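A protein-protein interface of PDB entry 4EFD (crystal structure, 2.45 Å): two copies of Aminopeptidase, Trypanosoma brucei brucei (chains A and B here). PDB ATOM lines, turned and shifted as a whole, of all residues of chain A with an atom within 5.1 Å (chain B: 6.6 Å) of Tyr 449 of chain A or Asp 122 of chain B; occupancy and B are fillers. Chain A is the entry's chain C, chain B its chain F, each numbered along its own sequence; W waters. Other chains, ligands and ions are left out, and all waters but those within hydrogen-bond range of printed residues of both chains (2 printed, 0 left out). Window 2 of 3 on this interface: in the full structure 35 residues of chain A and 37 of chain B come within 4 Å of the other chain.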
ATOM      1  N   CYS A 446     -24.748   7.390  -9.945  1.00  0.00           N
ATOM      2  CA  CYS A 446     -24.110   6.676  -8.846  1.00  0.00           C
ATOM      3  C   CYS A 446     -22.586   6.808  -8.949  1.00  0.00           C
ATOM      4  O   CYS A 446     -21.906   5.863  -9.344  1.00  0.00           O
ATOM      5  CB  CYS A 446     -24.539   5.205  -8.855  1.00  0.00           C
ATOM      6  SG  CYS A 446     -24.196   4.339  -7.325  1.00  0.00           S
ATOM      7  N   PRO A 447     -22.049   7.993  -8.596  1.00  0.00           N
ATOM      8  CA  PRO A 447     -20.616   8.283  -8.717  1.00  0.00           C
ATOM      9  C   PRO A 447     -19.684   7.309  -7.988  1.00  0.00           C
ATOM     10  O   PRO A 447     -18.529   7.170  -8.385  1.00  0.00           O
ATOM     11  CB  PRO A 447     -20.490   9.686  -8.111  1.00  0.00           C
ATOM     12  CG  PRO A 447     -21.824  10.290  -8.286  1.00  0.00           C
ATOM     13  CD  PRO A 447     -22.798   9.169  -8.117  1.00  0.00           C
ATOM     14  N   GLU A 448     -20.176   6.654  -6.936  1.00  0.00           N
ATOM     15  CA  GLU A 448     -19.382   5.656  -6.203  1.00  0.00           C
ATOM     16  C   GLU A 448     -18.902   4.547  -7.136  1.00  0.00           C
ATOM     17  O   GLU A 448     -17.767   4.087  -7.021  1.00  0.00           O
ATOM     18  CB  GLU A 448     -20.176   5.004  -5.062  1.00  0.00           C
ATOM     19  CG  GLU A 448     -20.978   5.943  -4.175  1.00  0.00           C
ATOM     20  CD  GLU A 448     -22.401   6.124  -4.660  1.00  0.00           C
ATOM     21  OE1 GLU A 448     -23.308   5.441  -4.139  1.00  0.00           O
ATOM     22  OE2 GLU A 448     -22.605   6.941  -5.577  1.00  0.00           O
ATOM     23  N   TYR A 449     -19.780   4.124  -8.045  1.00  0.00           N
ATOM     24  CA  TYR A 449     -19.503   3.006  -8.949  1.00  0.00           C
ATOM     25  C   TYR A 449     -18.921   3.425 -10.302  1.00  0.00           C
ATOM     26  O   TYR A 449     -18.363   2.590 -11.019  1.00  0.00           O
ATOM     27  CB  TYR A 449     -20.778   2.182  -9.175  1.00  0.00           C
ATOM     28  CG  TYR A 449     -21.381   1.566  -7.923  1.00  0.00           C
ATOM     29  CD1 TYR A 449     -20.579   1.118  -6.872  1.00  0.00           C
ATOM     30  CD2 TYR A 449     -22.757   1.397  -7.808  1.00  0.00           C
ATOM     31  CE1 TYR A 449     -21.136   0.548  -5.738  1.00  0.00           C
ATOM     32  CE2 TYR A 449     -23.323   0.824  -6.676  1.00  0.00           C
ATOM     33  CZ  TYR A 449     -22.507   0.401  -5.646  1.00  0.00           C
ATOM     34  OH  TYR A 449     -23.063  -0.171  -4.525  1.00  0.00           O
ATOM     35  N   HIS A 450     -19.044   4.705 -10.648  1.00  0.00           N
ATOM     36  CA  HIS A 450     -18.503   5.215 -11.910  1.00  0.00           C
ATOM     37  C   HIS A 450     -17.018   5.568 -11.797  1.00  0.00           C
ATOM     38  O   HIS A 450     -16.262   5.388 -12.755  1.00  0.00           O
ATOM     39  CB  HIS A 450     -19.290   6.439 -12.382  1.00  0.00           C
ATOM     40  CG  HIS A 450     -20.768   6.214 -12.459  1.00  0.00           C
ATOM     41  ND1 HIS A 450     -21.317   4.997 -12.802  1.00  0.00           N
ATOM     42  CD2 HIS A 450     -21.811   7.052 -12.249  1.00  0.00           C
ATOM     43  CE1 HIS A 450     -22.634   5.093 -12.789  1.00  0.00           C
ATOM     44  NE2 HIS A 450     -22.959   6.329 -12.456  1.00  0.00           N
ATOM     45  N   GLU A 451     -16.613   6.067 -10.628  1.00  0.00           N
ATOM     46  CA  GLU A 451     -15.237   6.522 -10.391  1.00  0.00           C
ATOM     47  C   GLU A 451     -14.161   5.457 -10.665  1.00  0.00           C
ATOM     48  O   GLU A 451     -13.161   5.760 -11.317  1.00  0.00           O
ATOM     49  CB  GLU A 451     -15.101   7.075  -8.961  1.00  0.00           C
ATOM     50  CG  GLU A 451     -13.703   7.568  -8.580  1.00  0.00           C
ATOM     51  CD  GLU A 451     -13.616   8.047  -7.136  1.00  0.00           C
ATOM     52  OE1 GLU A 451     -12.486   8.126  -6.604  1.00  0.00           O
ATOM     53  OE2 GLU A 451     -14.671   8.341  -6.526  1.00  0.00           O
ATOM     54  N   PRO A 452     -14.355   4.215 -10.172  1.00  0.00           N
ATOM     55  CA  PRO A 452     -13.348   3.163 -10.385  1.00  0.00           C
ATOM     56  C   PRO A 452     -13.074   2.813 -11.853  1.00  0.00           C
ATOM     57  O   PRO A 452     -11.972   2.369 -12.177  1.00  0.00           O
ATOM     58  CB  PRO A 452     -13.942   1.950  -9.656  1.00  0.00           C
ATOM     59  CG  PRO A 452     -14.889   2.518  -8.669  1.00  0.00           C
ATOM     60  CD  PRO A 452     -15.463   3.730  -9.328  1.00  0.00           C
ATOM     61  N   GLU A 453     -14.058   3.012 -12.728  1.00  0.00           N
ATOM     62  CA  GLU A 453     -13.894   2.719 -14.156  1.00  0.00           C
ATOM     63  C   GLU A 453     -12.870   3.618 -14.859  1.00  0.00           C
ATOM     64  O   GLU A 453     -12.348   3.246 -15.909  1.00  0.00           O
ATOM     65  CB  GLU A 453     -15.237   2.826 -14.887  1.00  0.00           C
ATOM     66  CG  GLU A 453     -16.266   1.769 -14.490  1.00  0.00           C
ATOM     67  CD  GLU A 453     -15.828   0.350 -14.824  1.00  0.00           C
ATOM     68  OE1 GLU A 453     -16.287  -0.584 -14.137  1.00  0.00           O
ATOM     69  OE2 GLU A 453     -15.028   0.163 -15.767  1.00  0.00           O
ATOM     70  N   ASN A 470     -20.865  -1.222 -17.817  1.00  0.00           N
ATOM     71  CA  ASN A 470     -21.073  -0.735 -16.453  1.00  0.00           C
ATOM     72  C   ASN A 470     -21.625   0.698 -16.440  1.00  0.00           C
ATOM     73  O   ASN A 470     -21.009   1.616 -15.891  1.00  0.00           O
ATOM     74  CB  ASN A 470     -19.769  -0.834 -15.649  1.00  0.00           C
ATOM     75  CG  ASN A 470     -19.992  -0.727 -14.145  1.00  0.00           C
ATOM     76  OD1 ASN A 470     -21.099  -0.945 -13.648  1.00  0.00           O
ATOM     77  ND2 ASN A 470     -18.933  -0.396 -13.413  1.00  0.00           N
ATOM     78  N   PRO B 109     -17.433   3.426   3.673  1.00  0.00           N
ATOM     79  CA  PRO B 109     -17.701   4.824   3.326  1.00  0.00           C
ATOM     80  C   PRO B 109     -19.136   5.245   3.636  1.00  0.00           C
ATOM     81  O   PRO B 109     -20.041   4.405   3.612  1.00  0.00           O
ATOM     82  CB  PRO B 109     -17.463   4.855   1.813  1.00  0.00           C
ATOM     83  CG  PRO B 109     -17.755   3.481   1.364  1.00  0.00           C
ATOM     84  CD  PRO B 109     -17.284   2.585   2.471  1.00  0.00           C
ATOM     85  N   ASN B 115     -29.572   6.665  -5.523  1.00  0.00           N
ATOM     86  CA  ASN B 115     -29.946   5.377  -6.109  1.00  0.00           C
ATOM     87  C   ASN B 115     -29.274   4.173  -5.433  1.00  0.00           C
ATOM     88  O   ASN B 115     -29.425   3.043  -5.896  1.00  0.00           O
ATOM     89  CB  ASN B 115     -29.608   5.375  -7.600  1.00  0.00           C
ATOM     90  CG  ASN B 115     -30.320   6.473  -8.357  1.00  0.00           C
ATOM     91  OD1 ASN B 115     -31.546   6.568  -8.324  1.00  0.00           O
ATOM     92  ND2 ASN B 115     -29.556   7.307  -9.046  1.00  0.00           N
ATOM     93  N   ASN B 116     -28.547   4.411  -4.342  1.00  0.00           N
ATOM     94  CA  ASN B 116     -27.812   3.350  -3.649  1.00  0.00           C
ATOM     95  C   ASN B 116     -28.350   3.125  -2.232  1.00  0.00           C
ATOM     96  O   ASN B 116     -29.172   3.899  -1.736  1.00  0.00           O
ATOM     97  CB  ASN B 116     -26.316   3.695  -3.606  1.00  0.00           C
ATOM     98  CG  ASN B 116     -25.416   2.460  -3.538  1.00  0.00           C
ATOM     99  OD1 ASN B 116     -25.884   1.338  -3.350  1.00  0.00           O
ATOM    100  ND2 ASN B 116     -24.116   2.674  -3.691  1.00  0.00           N
ATOM    101  N   CYS B 117     -27.895   2.046  -1.598  1.00  0.00           N
ATOM    102  CA  CYS B 117     -28.219   1.760  -0.201  1.00  0.00           C
ATOM    103  C   CYS B 117     -27.282   2.565   0.708  1.00  0.00           C
ATOM    104  O   CYS B 117     -26.063   2.430   0.600  1.00  0.00           O
ATOM    105  CB  CYS B 117     -28.073   0.262   0.075  1.00  0.00           C
ATOM    106  SG  CYS B 117     -28.281  -0.222   1.802  1.00  0.00           S
ATOM    107  N   ALA B 119     -26.317   2.295   3.741  1.00  0.00           N
ATOM    108  CA  ALA B 119     -25.410   1.488   4.561  1.00  0.00           C
ATOM    109  C   ALA B 119     -24.236   0.900   3.769  1.00  0.00           C
ATOM    110  O   ALA B 119     -23.302   0.365   4.365  1.00  0.00           O
ATOM    111  CB  ALA B 119     -26.183   0.373   5.254  1.00  0.00           C
ATOM    112  N   ARG B 120     -24.294   0.995   2.440  1.00  0.00           N
ATOM    113  CA  ARG B 120     -23.224   0.516   1.556  1.00  0.00           C
ATOM    114  C   ARG B 120     -22.807  -0.931   1.847  1.00  0.00           C
ATOM    115  O   ARG B 120     -21.639  -1.195   2.135  1.00  0.00           O
ATOM    116  CB  ARG B 120     -22.004   1.447   1.624  1.00  0.00           C
ATOM    117  CG  ARG B 120     -22.248   2.869   1.118  1.00  0.00           C
ATOM    118  CD  ARG B 120     -22.573   2.917  -0.376  1.00  0.00           C
ATOM    119  NE  ARG B 120     -21.556   2.262  -1.201  1.00  0.00           N
ATOM    120  CZ  ARG B 120     -20.422   2.825  -1.619  1.00  0.00           C
ATOM    121  NH1 ARG B 120     -20.117   4.079  -1.300  1.00  0.00           N
ATOM    122  NH2 ARG B 120     -19.577   2.120  -2.367  1.00  0.00           N
ATOM    123  N   PRO B 121     -23.762  -1.875   1.763  1.00  0.00           N
ATOM    124  CA  PRO B 121     -23.462  -3.292   1.993  1.00  0.00           C
ATOM    125  C   PRO B 121     -22.521  -3.903   0.950  1.00  0.00           C
ATOM    126  O   PRO B 121     -21.945  -4.961   1.192  1.00  0.00           O
ATOM    127  CB  PRO B 121     -24.841  -3.959   1.927  1.00  0.00           C
ATOM    128  CG  PRO B 121     -25.675  -3.034   1.129  1.00  0.00           C
ATOM    129  CD  PRO B 121     -25.187  -1.664   1.454  1.00  0.00           C
ATOM    130  N   ASP B 122     -22.381  -3.247  -0.200  1.00  0.00           N
ATOM    131  CA  ASP B 122     -21.404  -3.661  -1.205  1.00  0.00           C
ATOM    132  C   ASP B 122     -19.980  -3.649  -0.643  1.00  0.00           C
ATOM    133  O   ASP B 122     -19.208  -4.576  -0.887  1.00  0.00           O
ATOM    134  CB  ASP B 122     -21.491  -2.774  -2.456  1.00  0.00           C
ATOM    135  CG  ASP B 122     -21.174  -1.312  -2.169  1.00  0.00           C
ATOM    136  OD1 ASP B 122     -21.928  -0.673  -1.407  1.00  0.00           O
ATOM    137  OD2 ASP B 122     -20.175  -0.799  -2.709  1.00  0.00           O
ATOM    138  N   VAL B 123     -19.644  -2.612   0.124  1.00  0.00           N
ATOM    139  CA  VAL B 123     -18.310  -2.486   0.706  1.00  0.00           C
ATOM    140  C   VAL B 123     -18.157  -3.403   1.923  1.00  0.00           C
ATOM    141  O   VAL B 123     -17.087  -3.966   2.148  1.00  0.00           O
ATOM    142  CB  VAL B 123     -17.991  -1.026   1.095  1.00  0.00           C
ATOM    143  CG1 VAL B 123     -16.608  -0.926   1.732  1.00  0.00           C
ATOM    144  CG2 VAL B 123     -18.078  -0.121  -0.126  1.00  0.00           C
ATOM    145  N   VAL B 124     -19.228  -3.560   2.698  1.00  0.00           N
ATOM    146  CA  VAL B 124     -19.227  -4.492   3.828  1.00  0.00           C
ATOM    147  C   VAL B 124     -18.877  -5.914   3.376  1.00  0.00           C
ATOM    148  O   VAL B 124     -18.101  -6.604   4.041  1.00  0.00           O
ATOM    149  CB  VAL B 124     -20.585  -4.500   4.562  1.00  0.00           C
ATOM    150  CG1 VAL B 124     -20.621  -5.600   5.616  1.00  0.00           C
ATOM    151  CG2 VAL B 124     -20.851  -3.142   5.203  1.00  0.00           C
ATOM    152  N   THR B 125     -19.437  -6.343   2.246  1.00  0.00           N
ATOM    153  CA  THR B 125     -19.115  -7.650   1.668  1.00  0.00           C
ATOM    154  C   THR B 125     -17.627  -7.750   1.331  1.00  0.00           C
ATOM    155  O   THR B 125     -16.968  -8.728   1.688  1.00  0.00           O
ATOM    156  CB  THR B 125     -19.936  -7.931   0.389  1.00  0.00           C
ATOM    157  OG1 THR B 125     -21.338  -7.897   0.691  1.00  0.00           O
ATOM    158  CG2 THR B 125     -19.578  -9.295  -0.193  1.00  0.00           C
ATOM    159  N   ALA B 126     -17.110  -6.729   0.651  1.00  0.00           N
ATOM    160  CA  ALA B 126     -15.697  -6.679   0.261  1.00  0.00           C
ATOM    161  C   ALA B 126     -14.758  -6.708   1.467  1.00  0.00           C
ATOM    162  O   ALA B 126     -13.747  -7.410   1.451  1.00  0.00           O
ATOM    163  CB  ALA B 126     -15.425  -5.440  -0.582  1.00  0.00           C
ATOM    164  N   LEU B 127     -15.099  -5.944   2.503  1.00  0.00           N
ATOM    165  CA  LEU B 127     -14.268  -5.836   3.705  1.00  0.00           C
ATOM    166  C   LEU B 127     -14.177  -7.160   4.461  1.00  0.00           C
ATOM    167  O   LEU B 127     -13.089  -7.581   4.855  1.00  0.00           O
ATOM    168  CB  LEU B 127     -14.811  -4.742   4.637  1.00  0.00           C
ATOM    169  CG  LEU B 127     -14.707  -3.305   4.111  1.00  0.00           C
ATOM    170  CD1 LEU B 127     -15.610  -2.371   4.904  1.00  0.00           C
ATOM    171  CD2 LEU B 127     -13.272  -2.813   4.135  1.00  0.00           C
ATOM    172  N   ALA B 157     -25.396  -9.065   2.937  1.00  0.00           N
ATOM    173  CA  ALA B 157     -24.000  -8.750   2.614  1.00  0.00           C
ATOM    174  C   ALA B 157     -23.010  -9.778   3.160  1.00  0.00           C
ATOM    175  O   ALA B 157     -22.079 -10.177   2.463  1.00  0.00           O
ATOM    176  CB  ALA B 157     -23.638  -7.361   3.129  1.00  0.00           C
ATOM    177  N   ARG B 160     -23.297 -13.118   1.557  1.00  0.00           N
ATOM    178  CA  ARG B 160     -22.714 -12.990   0.226  1.00  0.00           C
ATOM    179  C   ARG B 160     -21.190 -13.126   0.207  1.00  0.00           C
ATOM    180  O   ARG B 160     -20.610 -13.506  -0.811  1.00  0.00           O
ATOM    181  CB  ARG B 160     -23.058 -11.605  -0.326  1.00  0.00           C
ATOM    182  CG  ARG B 160     -23.580 -11.611  -1.719  1.00  0.00           C
ATOM    183  CD  ARG B 160     -23.688 -10.201  -2.278  1.00  0.00           C
ATOM    184  NE  ARG B 160     -24.558  -9.349  -1.471  1.00  0.00           N
ATOM    185  CZ  ARG B 160     -25.891  -9.417  -1.444  1.00  0.00           C
ATOM    186  NH1 ARG B 160     -26.569  -8.581  -0.664  1.00  0.00           N
ATOM    187  NH2 ARG B 160     -26.556 -10.307  -2.180  1.00  0.00           N
ATOM    188  N   HIS B 414     -24.141  -3.211 -10.726  1.00  0.00           N
ATOM    189  CA  HIS B 414     -24.734  -3.248  -9.387  1.00  0.00           C
ATOM    190  C   HIS B 414     -26.237  -2.975  -9.350  1.00  0.00           C
ATOM    191  O   HIS B 414     -26.875  -3.216  -8.326  1.00  0.00           O
ATOM    192  CB  HIS B 414     -24.024  -2.242  -8.480  1.00  0.00           C
ATOM    193  CG  HIS B 414     -22.576  -2.546  -8.264  1.00  0.00           C
ATOM    194  ND1 HIS B 414     -21.591  -2.130  -9.134  1.00  0.00           N
ATOM    195  CD2 HIS B 414     -21.946  -3.233  -7.282  1.00  0.00           C
ATOM    196  CE1 HIS B 414     -20.416  -2.545  -8.695  1.00  0.00           C
ATOM    197  NE2 HIS B 414     -20.604  -3.216  -7.573  1.00  0.00           N
ATOM    198  N   HIS B 415     -26.799  -2.473 -10.449  1.00  0.00           N
ATOM    199  CA  HIS B 415     -28.213  -2.099 -10.491  1.00  0.00           C
ATOM    200  C   HIS B 415     -28.973  -2.901 -11.539  1.00  0.00           C
ATOM    201  O   HIS B 415     -28.685  -2.803 -12.731  1.00  0.00           O
ATOM    202  CB  HIS B 415     -28.360  -0.605 -10.785  1.00  0.00           C
ATOM    203  CG  HIS B 415     -27.897   0.277  -9.668  1.00  0.00           C
ATOM    204  ND1 HIS B 415     -26.577   0.631  -9.498  1.00  0.00           N
ATOM    205  CD2 HIS B 415     -28.579   0.876  -8.665  1.00  0.00           C
ATOM    206  CE1 HIS B 415     -26.465   1.409  -8.437  1.00  0.00           C
ATOM    207  NE2 HIS B 415     -27.666   1.573  -7.911  1.00  0.00           N
ATOM    208  N   GLY B 437     -30.253  -3.452  -0.296  1.00  0.00           N
ATOM    209  CA  GLY B 437     -28.887  -3.388  -0.813  1.00  0.00           C
ATOM    210  C   GLY B 437     -28.759  -4.008  -2.193  1.00  0.00           C
ATOM    211  O   GLY B 437     -27.768  -3.790  -2.890  1.00  0.00           O
ATOM    212  N   THR B 439     -29.712  -3.357  -5.194  1.00  0.00           N
ATOM    213  CA  THR B 439     -30.224  -2.137  -5.802  1.00  0.00           C
ATOM    214  C   THR B 439     -30.727  -2.327  -7.224  1.00  0.00           C
ATOM    215  O   THR B 439     -30.273  -3.215  -7.946  1.00  0.00           O
ATOM    216  CB  THR B 439     -29.141  -1.045  -5.809  1.00  0.00           C
ATOM    217  OG1 THR B 439     -27.940  -1.566  -6.394  1.00  0.00           O
ATOM    218  CG2 THR B 439     -28.849  -0.577  -4.394  1.00  0.00           C
HETATM  219  O   HOH W   1     -25.386  -1.476  -5.073  1.00  0.00           O
HETATM  220  O   HOH W   2     -24.597  -0.462  -1.856  1.00  0.00           O
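Among the printed residues, pairs that only touch across the chains: Cys 446 of chain A with Asn 116 of chain B (3.998 Å), Cys 446 of chain A with His 415 of chain B (3.9 Å), Glu 448 of chain A with Arg 120 of chain B (3.5 Å), Tyr 449 of chain A with His 414 of chain B (3.6 Å) and Tyr 449 of chain A with His 415 of chain B (3.6 Å).
Of the 19 printed residues of chain B, 5 touch a printed residue of chain A.
Printed residues of chain B that touch a printed residue of chain A: Asn 116, Arg 120, Asp 122, His 414 and His 415.
Hydrophobic or aromatic side chains of chain B within 4 Å of the printed part of chain A: His 414 and His 415.
The side-chain sulfur (SG) of Cys 446 of chain A is in hydrogen-bond range of the side-chain carboxylate (OE1) of Glu 448 of chain A (3.5 Å).
N of Cys 446 of chain A lies within hydrogen-bond range of NE2 of His 450 of chain A (3.3 Å).
O of Asn 115 of chain B sits at hydrogen-bond distance from NE2 of His 415 of chain B (3.1 Å).
NE of Arg 120 of chain B is in salt-bridge range of OD1 of Asp 122 of chain B, 3.0 Å away.
OG1 of Thr 439 of chain B sits at hydrogen-bond distance from O of His 414 of chain B (2.8 Å).
A ring nitrogen (NE2) of His 415 of chain B sits close to the side-chain hydroxyl of Thr 439 of chain B, 3.5 Å away.
Water W2 lies within hydrogen-bond range of the side-chain amide oxygen of Asn 116 of chain B, the side-chain carboxylate of Asp 122 of chain B and the side-chain hydroxyl of Tyr 449 of chain A.
Water W1 lies within hydrogen-bond range of OH of Tyr 449 of chain A, OG1 of Thr 439 of chain B and OD1 of Asn 116 of chain B.
No position is printed for both chains.
Of the 8 pairs that touch across the chains among the printed residues, none has its exchanged pair printed and touching as well.
Tyr 449 of chain A touches four residues of chain B.
Of chain A, only Tyr 449 (3.2 Å) comes within 4 Å of Asp 122 of chain B.
Of the printed residues of chain B, Cys 446 of chain A touches Asn 116 and His 415.
Of the printed residues of chain B, Glu 448 of chain A touches Asn 116 and Arg 120.
Printed residues of chain A within 4 Å of Asn 116 of chain B: Cys 446, Glu 448 and Tyr 449.
Of the printed residues of chain A, His 415 of chain B touches Cys 446 (3.9 Å) and Tyr 449 (3.6 Å).
The nearest printed residue of chain A that does not touch Asp 122 of chain B is Glu 448 of chain A (6.3 Å).
The side-chain carboxylate of Glu 448 of chain A lies within hydrogen-bond range of the side-chain amide nitrogen of Asn 116 of chain B, 2.9 Å away.
The side-chain amide nitrogen of Asn 116 of chain B is in hydrogen-bond range of the side-chain hydroxyl of Tyr 449 of chain A, 3.1 Å away.
The side-chain carboxylate (OD1) of Asp 122 of chain B sits close to the side-chain hydroxyl (OH) of Tyr 449 of chain A, at 3.4 Å.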
